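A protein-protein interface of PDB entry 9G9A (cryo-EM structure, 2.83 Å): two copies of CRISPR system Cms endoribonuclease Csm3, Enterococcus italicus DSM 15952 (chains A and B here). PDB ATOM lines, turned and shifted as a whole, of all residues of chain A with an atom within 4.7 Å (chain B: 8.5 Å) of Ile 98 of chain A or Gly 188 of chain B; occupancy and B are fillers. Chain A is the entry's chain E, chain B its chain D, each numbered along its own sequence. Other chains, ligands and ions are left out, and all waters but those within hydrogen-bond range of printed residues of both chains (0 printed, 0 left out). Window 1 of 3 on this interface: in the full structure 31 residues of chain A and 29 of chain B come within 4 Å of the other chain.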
ATOM      1  N   GLY A  48     -21.113  21.674 -17.037  1.00  0.00           N
ATOM      2  CA  GLY A  48     -21.861  22.658 -16.274  1.00  0.00           C
ATOM      3  C   GLY A  48     -21.698  24.061 -16.825  1.00  0.00           C
ATOM      4  O   GLY A  48     -22.540  24.931 -16.592  1.00  0.00           O
ATOM      5  N   ILE A  51     -24.575  24.554 -19.304  1.00  0.00           N
ATOM      6  CA  ILE A  51     -25.836  24.727 -18.590  1.00  0.00           C
ATOM      7  C   ILE A  51     -25.922  26.122 -17.988  1.00  0.00           C
ATOM      8  O   ILE A  51     -26.920  26.832 -18.171  1.00  0.00           O
ATOM      9  CB  ILE A  51     -25.991  23.643 -17.509  1.00  0.00           C
ATOM     10  CG1 ILE A  51     -25.765  22.249 -18.097  1.00  0.00           C
ATOM     11  CG2 ILE A  51     -27.361  23.731 -16.860  1.00  0.00           C
ATOM     12  CD1 ILE A  51     -25.830  21.140 -17.071  1.00  0.00           C
ATOM     13  N   LYS A  52     -24.879  26.539 -17.263  1.00  0.00           N
ATOM     14  CA  LYS A  52     -24.904  27.851 -16.630  1.00  0.00           C
ATOM     15  C   LYS A  52     -24.973  28.962 -17.668  1.00  0.00           C
ATOM     16  O   LYS A  52     -25.721  29.932 -17.497  1.00  0.00           O
ATOM     17  CB  LYS A  52     -23.679  28.036 -15.736  1.00  0.00           C
ATOM     18  CG  LYS A  52     -23.730  29.312 -14.910  1.00  0.00           C
ATOM     19  CD  LYS A  52     -22.414  29.601 -14.227  1.00  0.00           C
ATOM     20  CE  LYS A  52     -22.505  30.859 -13.386  1.00  0.00           C
ATOM     21  NZ  LYS A  52     -21.177  31.288 -12.879  1.00  0.00           N
ATOM     22  N   MET A  55     -28.532  29.045 -19.253  1.00  0.00           N
ATOM     23  CA  MET A  55     -29.492  29.565 -18.285  1.00  0.00           C
ATOM     24  C   MET A  55     -29.320  31.069 -18.098  1.00  0.00           C
ATOM     25  O   MET A  55     -30.304  31.818 -18.067  1.00  0.00           O
ATOM     26  CB  MET A  55     -29.343  28.833 -16.952  1.00  0.00           C
ATOM     27  CG  MET A  55     -29.848  27.402 -16.963  1.00  0.00           C
ATOM     28  SD  MET A  55     -29.565  26.567 -15.391  1.00  0.00           S
ATOM     29  CE  MET A  55     -30.425  27.664 -14.269  1.00  0.00           C
ATOM     30  N   LEU A  96     -25.189  30.352  -7.617  1.00  0.00           N
ATOM     31  CA  LEU A  96     -25.390  29.119  -8.363  1.00  0.00           C
ATOM     32  C   LEU A  96     -24.058  28.503  -8.770  1.00  0.00           C
ATOM     33  O   LEU A  96     -23.209  29.158  -9.382  1.00  0.00           O
ATOM     34  CB  LEU A  96     -26.237  29.378  -9.605  1.00  0.00           C
ATOM     35  CG  LEU A  96     -27.749  29.363  -9.398  1.00  0.00           C
ATOM     36  CD1 LEU A  96     -28.460  29.504 -10.728  1.00  0.00           C
ATOM     37  CD2 LEU A  96     -28.157  28.083  -8.698  1.00  0.00           C
ATOM     38  N   GLN A  97     -23.881  27.228  -8.427  1.00  0.00           N
ATOM     39  CA  GLN A  97     -22.745  26.427  -8.864  1.00  0.00           C
ATOM     40  C   GLN A  97     -23.309  25.203  -9.583  1.00  0.00           C
ATOM     41  O   GLN A  97     -23.795  24.259  -8.956  1.00  0.00           O
ATOM     42  CB  GLN A  97     -21.855  26.028  -7.688  1.00  0.00           C
ATOM     43  CG  GLN A  97     -21.374  27.194  -6.849  1.00  0.00           C
ATOM     44  CD  GLN A  97     -20.568  26.750  -5.647  1.00  0.00           C
ATOM     45  OE1 GLN A  97     -20.206  27.557  -4.794  1.00  0.00           O
ATOM     46  NE2 GLN A  97     -20.283  25.456  -5.573  1.00  0.00           N
ATOM     47  N   ILE A  98     -23.266  25.243 -10.914  1.00  0.00           N
ATOM     48  CA  ILE A  98     -23.815  24.160 -11.715  1.00  0.00           C
ATOM     49  C   ILE A  98     -22.686  23.247 -12.170  1.00  0.00           C
ATOM     50  O   ILE A  98     -21.675  23.706 -12.716  1.00  0.00           O
ATOM     51  CB  ILE A  98     -24.595  24.729 -12.910  1.00  0.00           C
ATOM     52  CG1 ILE A  98     -25.638  25.733 -12.415  1.00  0.00           C
ATOM     53  CG2 ILE A  98     -25.247  23.610 -13.696  1.00  0.00           C
ATOM     54  CD1 ILE A  98     -26.428  26.390 -13.512  1.00  0.00           C
ATOM     55  N   SER A  99     -22.854  21.948 -11.946  1.00  0.00           N
ATOM     56  CA  SER A  99     -21.800  20.976 -12.184  1.00  0.00           C
ATOM     57  C   SER A  99     -22.012  20.288 -13.522  1.00  0.00           C
ATOM     58  O   SER A  99     -23.077  20.390 -14.137  1.00  0.00           O
ATOM     59  CB  SER A  99     -21.745  19.927 -11.073  1.00  0.00           C
ATOM     60  OG  SER A  99     -20.773  18.938 -11.359  1.00  0.00           O
ATOM     61  N   ASP A 100     -20.972  19.589 -13.967  1.00  0.00           N
ATOM     62  CA  ASP A 100     -21.065  18.783 -15.175  1.00  0.00           C
ATOM     63  C   ASP A 100     -22.092  17.677 -14.987  1.00  0.00           C
ATOM     64  O   ASP A 100     -22.103  16.990 -13.962  1.00  0.00           O
ATOM     65  CB  ASP A 100     -19.700  18.182 -15.516  1.00  0.00           C
ATOM     66  CG  ASP A 100     -18.631  19.238 -15.717  1.00  0.00           C
ATOM     67  OD1 ASP A 100     -18.965  20.359 -16.149  1.00  0.00           O
ATOM     68  OD2 ASP A 100     -17.450  18.941 -15.445  1.00  0.00           O
ATOM     69  N   HIS A 151     -26.336  18.218 -10.909  1.00  0.00           N
ATOM     70  CA  HIS A 151     -26.128  18.558  -9.507  1.00  0.00           C
ATOM     71  C   HIS A 151     -25.807  20.041  -9.418  1.00  0.00           C
ATOM     72  O   HIS A 151     -24.800  20.491  -9.973  1.00  0.00           O
ATOM     73  CB  HIS A 151     -24.995  17.715  -8.914  1.00  0.00           C
ATOM     74  CG  HIS A 151     -24.499  18.205  -7.591  1.00  0.00           C
ATOM     75  ND1 HIS A 151     -23.531  19.180  -7.474  1.00  0.00           N
ATOM     76  CD2 HIS A 151     -24.821  17.843  -6.327  1.00  0.00           C
ATOM     77  CE1 HIS A 151     -23.288  19.404  -6.195  1.00  0.00           C
ATOM     78  NE2 HIS A 151     -24.056  18.604  -5.478  1.00  0.00           N
ATOM     79  N   ILE A 152     -26.656  20.797  -8.726  1.00  0.00           N
ATOM     80  CA  ILE A 152     -26.528  22.245  -8.617  1.00  0.00           C
ATOM     81  C   ILE A 152     -26.484  22.608  -7.140  1.00  0.00           C
ATOM     82  O   ILE A 152     -27.215  22.026  -6.331  1.00  0.00           O
ATOM     83  CB  ILE A 152     -27.689  22.969  -9.324  1.00  0.00           C
ATOM     84  CG1 ILE A 152     -27.753  22.561 -10.797  1.00  0.00           C
ATOM     85  CG2 ILE A 152     -27.539  24.476  -9.201  1.00  0.00           C
ATOM     86  CD1 ILE A 152     -28.835  23.271 -11.579  1.00  0.00           C
ATOM     87  N   VAL B  13     -11.376  13.676  -7.474  1.00  0.00           N
ATOM     88  CA  VAL B  13     -11.749  14.761  -8.375  1.00  0.00           C
ATOM     89  C   VAL B  13     -13.084  14.384  -9.012  1.00  0.00           C
ATOM     90  O   VAL B  13     -13.125  13.736 -10.052  1.00  0.00           O
ATOM     91  CB  VAL B  13     -10.665  15.009  -9.423  1.00  0.00           C
ATOM     92  CG1 VAL B  13     -11.016  16.188 -10.299  1.00  0.00           C
ATOM     93  CG2 VAL B  13      -9.327  15.235  -8.747  1.00  0.00           C
ATOM     94  N   LEU B  14     -14.189  14.795  -8.381  1.00  0.00           N
ATOM     95  CA  LEU B  14     -15.508  14.445  -8.903  1.00  0.00           C
ATOM     96  C   LEU B  14     -15.749  15.068 -10.272  1.00  0.00           C
ATOM     97  O   LEU B  14     -16.271  14.410 -11.179  1.00  0.00           O
ATOM     98  CB  LEU B  14     -16.597  14.873  -7.918  1.00  0.00           C
ATOM     99  CG  LEU B  14     -16.532  14.245  -6.527  1.00  0.00           C
ATOM    100  CD1 LEU B  14     -17.758  14.614  -5.716  1.00  0.00           C
ATOM    101  CD2 LEU B  14     -16.386  12.739  -6.624  1.00  0.00           C
ATOM    102  N   THR B  15     -15.386  16.338 -10.438  1.00  0.00           N
ATOM    103  CA  THR B  15     -15.412  17.007 -11.730  1.00  0.00           C
ATOM    104  C   THR B  15     -14.073  17.699 -11.940  1.00  0.00           C
ATOM    105  O   THR B  15     -13.377  18.022 -10.976  1.00  0.00           O
ATOM    106  CB  THR B  15     -16.553  18.035 -11.836  1.00  0.00           C
ATOM    107  OG1 THR B  15     -16.274  19.155 -10.990  1.00  0.00           O
ATOM    108  CG2 THR B  15     -17.877  17.417 -11.423  1.00  0.00           C
ATOM    109  N   GLY B  16     -13.732  17.933 -13.208  1.00  0.00           N
ATOM    110  CA  GLY B  16     -12.434  18.457 -13.601  1.00  0.00           C
ATOM    111  C   GLY B  16     -11.861  19.549 -12.721  1.00  0.00           C
ATOM    112  O   GLY B  16     -12.521  20.558 -12.456  1.00  0.00           O
ATOM    113  N   LEU B  17     -10.627  19.358 -12.265  1.00  0.00           N
ATOM    114  CA  LEU B  17      -9.981  20.253 -11.316  1.00  0.00           C
ATOM    115  C   LEU B  17      -8.967  21.122 -12.043  1.00  0.00           C
ATOM    116  O   LEU B  17      -8.088  20.607 -12.741  1.00  0.00           O
ATOM    117  CB  LEU B  17      -9.292  19.460 -10.206  1.00  0.00           C
ATOM    118  CG  LEU B  17      -8.508  20.266  -9.174  1.00  0.00           C
ATOM    119  CD1 LEU B  17      -9.444  21.101  -8.319  1.00  0.00           C
ATOM    120  CD2 LEU B  17      -7.675  19.340  -8.317  1.00  0.00           C
ATOM    121  N   HIS B  18      -9.088  22.436 -11.876  1.00  0.00           N
ATOM    122  CA  HIS B  18      -8.198  23.397 -12.515  1.00  0.00           C
ATOM    123  C   HIS B  18      -7.669  24.356 -11.459  1.00  0.00           C
ATOM    124  O   HIS B  18      -8.423  25.182 -10.936  1.00  0.00           O
ATOM    125  CB  HIS B  18      -8.925  24.159 -13.626  1.00  0.00           C
ATOM    126  CG  HIS B  18      -8.053  25.119 -14.374  1.00  0.00           C
ATOM    127  ND1 HIS B  18      -6.682  25.140 -14.241  1.00  0.00           N
ATOM    128  CD2 HIS B  18      -8.359  26.094 -15.264  1.00  0.00           C
ATOM    129  CE1 HIS B  18      -6.180  26.086 -15.014  1.00  0.00           C
ATOM    130  NE2 HIS B  18      -7.177  26.678 -15.647  1.00  0.00           N
ATOM    131  N   GLU B 120      -6.855  16.838 -19.029  1.00  0.00           N
ATOM    132  CA  GLU B 120      -7.684  17.019 -20.210  1.00  0.00           C
ATOM    133  C   GLU B 120      -7.722  18.496 -20.572  1.00  0.00           C
ATOM    134  O   GLU B 120      -7.449  19.367 -19.744  1.00  0.00           O
ATOM    135  CB  GLU B 120      -9.112  16.506 -19.982  1.00  0.00           C
ATOM    136  CG  GLU B 120      -9.779  17.103 -18.754  1.00  0.00           C
ATOM    137  CD  GLU B 120     -11.290  17.105 -18.850  1.00  0.00           C
ATOM    138  OE1 GLU B 120     -11.815  17.229 -19.976  1.00  0.00           O
ATOM    139  OE2 GLU B 120     -11.954  16.981 -17.800  1.00  0.00           O
ATOM    140  N   LYS B 122     -10.277  21.182 -21.591  1.00  0.00           N
ATOM    141  CA  LYS B 122     -11.670  21.578 -21.698  1.00  0.00           C
ATOM    142  C   LYS B 122     -11.780  22.786 -22.618  1.00  0.00           C
ATOM    143  O   LYS B 122     -11.101  23.800 -22.413  1.00  0.00           O
ATOM    144  CB  LYS B 122     -12.242  21.900 -20.317  1.00  0.00           C
ATOM    145  CG  LYS B 122     -13.739  22.157 -20.302  1.00  0.00           C
ATOM    146  CD  LYS B 122     -14.240  22.389 -18.888  1.00  0.00           C
ATOM    147  CE  LYS B 122     -15.758  22.449 -18.837  1.00  0.00           C
ATOM    148  NZ  LYS B 122     -16.305  23.604 -19.596  1.00  0.00           N
ATOM    149  N   GLU B 124     -14.036  25.771 -24.207  1.00  0.00           N
ATOM    150  CA  GLU B 124     -15.162  26.621 -23.871  1.00  0.00           C
ATOM    151  C   GLU B 124     -15.196  27.803 -24.826  1.00  0.00           C
ATOM    152  O   GLU B 124     -14.333  27.951 -25.693  1.00  0.00           O
ATOM    153  CB  GLU B 124     -15.070  27.124 -22.428  1.00  0.00           C
ATOM    154  CG  GLU B 124     -14.983  26.021 -21.396  1.00  0.00           C
ATOM    155  CD  GLU B 124     -14.150  26.417 -20.198  1.00  0.00           C
ATOM    156  OE1 GLU B 124     -13.081  27.033 -20.396  1.00  0.00           O
ATOM    157  OE2 GLU B 124     -14.565  26.116 -19.058  1.00  0.00           O
ATOM    158  N   ILE B 139      -8.871  25.366 -21.275  1.00  0.00           N
ATOM    159  CA  ILE B 139      -8.351  25.275 -19.915  1.00  0.00           C
ATOM    160  C   ILE B 139      -7.927  23.838 -19.647  1.00  0.00           C
ATOM    161  O   ILE B 139      -8.658  22.898 -19.973  1.00  0.00           O
ATOM    162  CB  ILE B 139      -9.378  25.745 -18.867  1.00  0.00           C
ATOM    163  CG1 ILE B 139     -10.710  25.014 -19.042  1.00  0.00           C
ATOM    164  CG2 ILE B 139      -9.579  27.249 -18.952  1.00  0.00           C
ATOM    165  CD1 ILE B 139     -11.675  25.232 -17.903  1.00  0.00           C
ATOM    166  N   ARG B 141      -7.465  20.743 -17.194  1.00  0.00           N
ATOM    167  CA  ARG B 141      -8.126  20.267 -15.990  1.00  0.00           C
ATOM    168  C   ARG B 141      -7.601  18.886 -15.637  1.00  0.00           C
ATOM    169  O   ARG B 141      -7.092  18.171 -16.501  1.00  0.00           O
ATOM    170  CB  ARG B 141      -9.652  20.213 -16.159  1.00  0.00           C
ATOM    171  CG  ARG B 141     -10.313  21.553 -16.413  1.00  0.00           C
ATOM    172  CD  ARG B 141     -11.801  21.478 -16.135  1.00  0.00           C
ATOM    173  NE  ARG B 141     -12.402  20.277 -16.699  1.00  0.00           N
ATOM    174  CZ  ARG B 141     -13.674  19.934 -16.549  1.00  0.00           C
ATOM    175  NH1 ARG B 141     -14.514  20.684 -15.855  1.00  0.00           N
ATOM    176  NH2 ARG B 141     -14.115  18.814 -17.108  1.00  0.00           N
ATOM    177  N   TYR B 180     -16.237  24.037  -4.422  1.00  0.00           N
ATOM    178  CA  TYR B 180     -15.188  23.584  -5.322  1.00  0.00           C
ATOM    179  C   TYR B 180     -13.821  23.825  -4.699  1.00  0.00           C
ATOM    180  O   TYR B 180     -13.716  24.247  -3.545  1.00  0.00           O
ATOM    181  CB  TYR B 180     -15.283  24.307  -6.664  1.00  0.00           C
ATOM    182  CG  TYR B 180     -15.280  25.810  -6.557  1.00  0.00           C
ATOM    183  CD1 TYR B 180     -16.456  26.508  -6.341  1.00  0.00           C
ATOM    184  CD2 TYR B 180     -14.105  26.533  -6.695  1.00  0.00           C
ATOM    185  CE1 TYR B 180     -16.464  27.879  -6.250  1.00  0.00           C
ATOM    186  CE2 TYR B 180     -14.102  27.908  -6.604  1.00  0.00           C
ATOM    187  CZ  TYR B 180     -15.286  28.574  -6.382  1.00  0.00           C
ATOM    188  OH  TYR B 180     -15.295  29.945  -6.291  1.00  0.00           O
ATOM    189  N   GLY B 182     -10.872  25.074  -6.877  1.00  0.00           N
ATOM    190  CA  GLY B 182     -10.263  26.214  -7.539  1.00  0.00           C
ATOM    191  C   GLY B 182     -10.550  26.248  -9.021  1.00  0.00           C
ATOM    192  O   GLY B 182     -10.875  25.227  -9.638  1.00  0.00           O
ATOM    193  N   GLY B 183     -10.430  27.445  -9.587  1.00  0.00           N
ATOM    194  CA  GLY B 183     -10.476  27.594 -11.038  1.00  0.00           C
ATOM    195  C   GLY B 183     -11.773  27.147 -11.667  1.00  0.00           C
ATOM    196  O   GLY B 183     -11.796  26.159 -12.411  1.00  0.00           O
ATOM    197  N   GLY B 184     -12.861  27.846 -11.375  1.00  0.00           N
ATOM    198  CA  GLY B 184     -14.145  27.478 -11.931  1.00  0.00           C
ATOM    199  C   GLY B 184     -15.196  27.330 -10.857  1.00  0.00           C
ATOM    200  O   GLY B 184     -15.558  28.302 -10.187  1.00  0.00           O
ATOM    201  N   GLY B 185     -15.695  26.108 -10.690  1.00  0.00           N
ATOM    202  CA  GLY B 185     -16.662  25.787  -9.671  1.00  0.00           C
ATOM    203  C   GLY B 185     -18.088  26.152 -10.014  1.00  0.00           C
ATOM    204  O   GLY B 185     -18.938  25.258 -10.096  1.00  0.00           O
ATOM    205  N   THR B 186     -18.374  27.439 -10.209  1.00  0.00           N
ATOM    206  CA  THR B 186     -19.723  27.835 -10.595  1.00  0.00           C
ATOM    207  C   THR B 186     -20.048  27.353 -12.003  1.00  0.00           C
ATOM    208  O   THR B 186     -21.220  27.296 -12.391  1.00  0.00           O
ATOM    209  CB  THR B 186     -19.875  29.351 -10.494  1.00  0.00           C
ATOM    210  OG1 THR B 186     -19.174  29.975 -11.575  1.00  0.00           O
ATOM    211  CG2 THR B 186     -19.305  29.853  -9.173  1.00  0.00           C
ATOM    212  N   ARG B 187     -19.024  26.996 -12.775  1.00  0.00           N
ATOM    213  CA  ARG B 187     -19.188  26.446 -14.113  1.00  0.00           C
ATOM    214  C   ARG B 187     -18.867  24.956 -14.186  1.00  0.00           C
ATOM    215  O   ARG B 187     -18.639  24.438 -15.284  1.00  0.00           O
ATOM    216  CB  ARG B 187     -18.321  27.221 -15.105  1.00  0.00           C
ATOM    217  CG  ARG B 187     -18.829  28.628 -15.378  1.00  0.00           C
ATOM    218  CD  ARG B 187     -17.872  29.417 -16.253  1.00  0.00           C
ATOM    219  NE  ARG B 187     -16.615  29.698 -15.569  1.00  0.00           N
ATOM    220  CZ  ARG B 187     -16.389  30.777 -14.835  1.00  0.00           C
ATOM    221  NH1 ARG B 187     -17.317  31.705 -14.668  1.00  0.00           N
ATOM    222  NH2 ARG B 187     -15.204  30.931 -14.252  1.00  0.00           N
ATOM    223  N   GLY B 188     -18.839  24.260 -13.050  1.00  0.00           N
ATOM    224  CA  GLY B 188     -18.729  22.818 -13.038  1.00  0.00           C
ATOM    225  C   GLY B 188     -17.356  22.255 -12.750  1.00  0.00           C
ATOM    226  O   GLY B 188     -17.199  21.028 -12.757  1.00  0.00           O
ATOM    227  N   ASN B 189     -16.357  23.094 -12.506  1.00  0.00           N
ATOM    228  CA  ASN B 189     -15.014  22.591 -12.262  1.00  0.00           C
ATOM    229  C   ASN B 189     -14.768  22.392 -10.770  1.00  0.00           C
ATOM    230  O   ASN B 189     -15.452  22.972  -9.924  1.00  0.00           O
ATOM    231  CB  ASN B 189     -13.973  23.555 -12.833  1.00  0.00           C
ATOM    232  CG  ASN B 189     -14.121  23.759 -14.326  1.00  0.00           C
ATOM    233  OD1 ASN B 189     -15.149  23.426 -14.916  1.00  0.00           O
ATOM    234  ND2 ASN B 189     -13.091  24.314 -14.947  1.00  0.00           N
ATOM    235  N   GLY B 190     -13.796  21.546 -10.452  1.00  0.00           N
ATOM    236  CA  GLY B 190     -13.223  21.512  -9.124  1.00  0.00           C
ATOM    237  C   GLY B 190     -14.000  20.772  -8.061  1.00  0.00           C
ATOM    238  O   GLY B 190     -13.584  20.798  -6.896  1.00  0.00           O
ATOM    239  N   ARG B 191     -15.107  20.119  -8.402  1.00  0.00           N
ATOM    240  CA  ARG B 191     -15.837  19.355  -7.399  1.00  0.00           C
ATOM    241  C   ARG B 191     -14.993  18.180  -6.930  1.00  0.00           C
ATOM    242  O   ARG B 191     -14.468  17.410  -7.738  1.00  0.00           O
ATOM    243  CB  ARG B 191     -17.173  18.868  -7.955  1.00  0.00           C
ATOM    244  CG  ARG B 191     -18.227  19.953  -8.020  1.00  0.00           C
ATOM    245  CD  ARG B 191     -19.595  19.400  -8.374  1.00  0.00           C
ATOM    246  NE  ARG B 191     -20.062  18.391  -7.430  1.00  0.00           N
ATOM    247  CZ  ARG B 191     -20.361  17.141  -7.756  1.00  0.00           C
ATOM    248  NH1 ARG B 191     -20.266  16.708  -9.001  1.00  0.00           N
ATOM    249  NH2 ARG B 191     -20.776  16.307  -6.807  1.00  0.00           N
ATOM    250  N   ILE B 192     -14.853  18.052  -5.611  1.00  0.00           N
ATOM    251  CA  ILE B 192     -13.972  17.062  -5.010  1.00  0.00           C
ATOM    252  C   ILE B 192     -14.668  16.417  -3.820  1.00  0.00           C
ATOM    253  O   ILE B 192     -15.641  16.941  -3.274  1.00  0.00           O
ATOM    254  CB  ILE B 192     -12.618  17.675  -4.580  1.00  0.00           C
ATOM    255  CG1 ILE B 192     -12.820  19.032  -3.901  1.00  0.00           C
ATOM    256  CG2 ILE B 192     -11.691  17.815  -5.779  1.00  0.00           C
ATOM    257  CD1 ILE B 192     -13.012  18.959  -2.403  1.00  0.00           C
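No position is printed for both chains. Of the 16 pairs that touch across the chains among the printed residues, none has its exchanged pair printed and touching as well.
Of the 11 printed residues of chain A, 8 touch a printed residue of chain B.
Gly 48 of chain A touches Arg 187 of chain B. Lys 52 of chain A touches Arg 187 of chain B (CD to CG, 3.9 Å). CB of Thr 186 of chain B touches O of Leu 96 of chain A, 3.5 Å away. O of Gly 185 of chain B touches CB of Gln 97 of chain A, 3.9 Å away. Gln 97 of chain A touches Thr 186 of chain B (CA to CA, 3.8 Å). Ile 98 of chain A touches Arg 187 of chain B. OG of Ser 99 of chain A touches CG2 of Thr 15 of chain B, at 3.3 Å. CA of Gly 188 of chain B touches CA of Ser 99 of chain A, at 3.7 Å. Thr 15 of chain B touches Asp 100 of chain A (CB to OD2, 3.8 Å). ND1 of His 151 of chain A touches NE of Arg 191 of chain B, at 3.6 Å.
Ile 98 of chain A touches three residues of chain B. Of chain A, only Ile 98, Ser 99 and Asp 100 come within 4 Å of Gly 188 of chain B. Of chain B, only Thr 15, Gly 188 and Arg 191 come within 4 Å of Ser 99 of chain A. Of the printed residues of chain A, Thr 15 of chain B touches Ser 99 (3.3 Å) and Asp 100 (3.8 Å). Of the printed residues of chain A, Arg 187 of chain B touches Gly 48 (3.4 Å), Lys 52 (3.9 Å) and Ile 98 (3.4 Å). Gly 16 of chain B touches none of the printed residues of chain A. The nearest residue of chain B that does not touch Ile 98 of chain A is Gly 185 of chain B (4.1 Å). The nearest printed residue of chain B that does not touch Gln 97 of chain A is Tyr 180 of chain B (4.03 Å).
The guanidinium group of Arg 141 of chain B is in salt-bridge range of the side-chain carboxylate of Asp 100 of chain A. NZ of Lys 52 of chain A lies within hydrogen-bond range of OG1 of Thr 186 of chain B (2.7 Å). The backbone carbonyl oxygen (O) of Thr 186 of chain B is in hydrogen-bond range of the backbone NH (N) of Ile 98 of chain A, 3.3 Å away. The backbone carbonyl oxygen of Ile 98 of chain A is in hydrogen-bond range of the backbone NH of Gly 188 of chain B, 2.9 Å away. The side-chain hydroxyl (OG) of Ser 99 of chain A lies close to the guanidinium group (NH1) of Arg 191 of chain B (3.3 Å). The side-chain carboxylate (OD2) of Asp 100 of chain A sits close to the backbone carbonyl oxygen (O) of Gly 188 of chain B, at 3.4 Å.
O of Arg 191 of chain B sits at hydrogen-bond distance from N of Leu 14 of chain B, 2.7 Å away. N of Gly 190 of chain B is in hydrogen-bond range of OG1 of Thr 15 of chain B (3.5 Å). The backbone NH of Arg 191 of chain B lies within hydrogen-bond range of the side-chain hydroxyl of Thr 15 of chain B. The side-chain carboxylate (OE2) of Glu 120 of chain B lies within salt-bridge range of the guanidinium group (NH2) of Arg 141 of chain B (2.9 Å). The guanidinium group (NH1) of Arg 141 of chain B lies within hydrogen-bond range of the side-chain amide oxygen (OD1) of Asn 189 of chain B (3.0 Å). The backbone carbonyl oxygen (O) of His 151 of chain A lies within hydrogen-bond range of the backbone NH (N) of Ser 99 of chain A.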
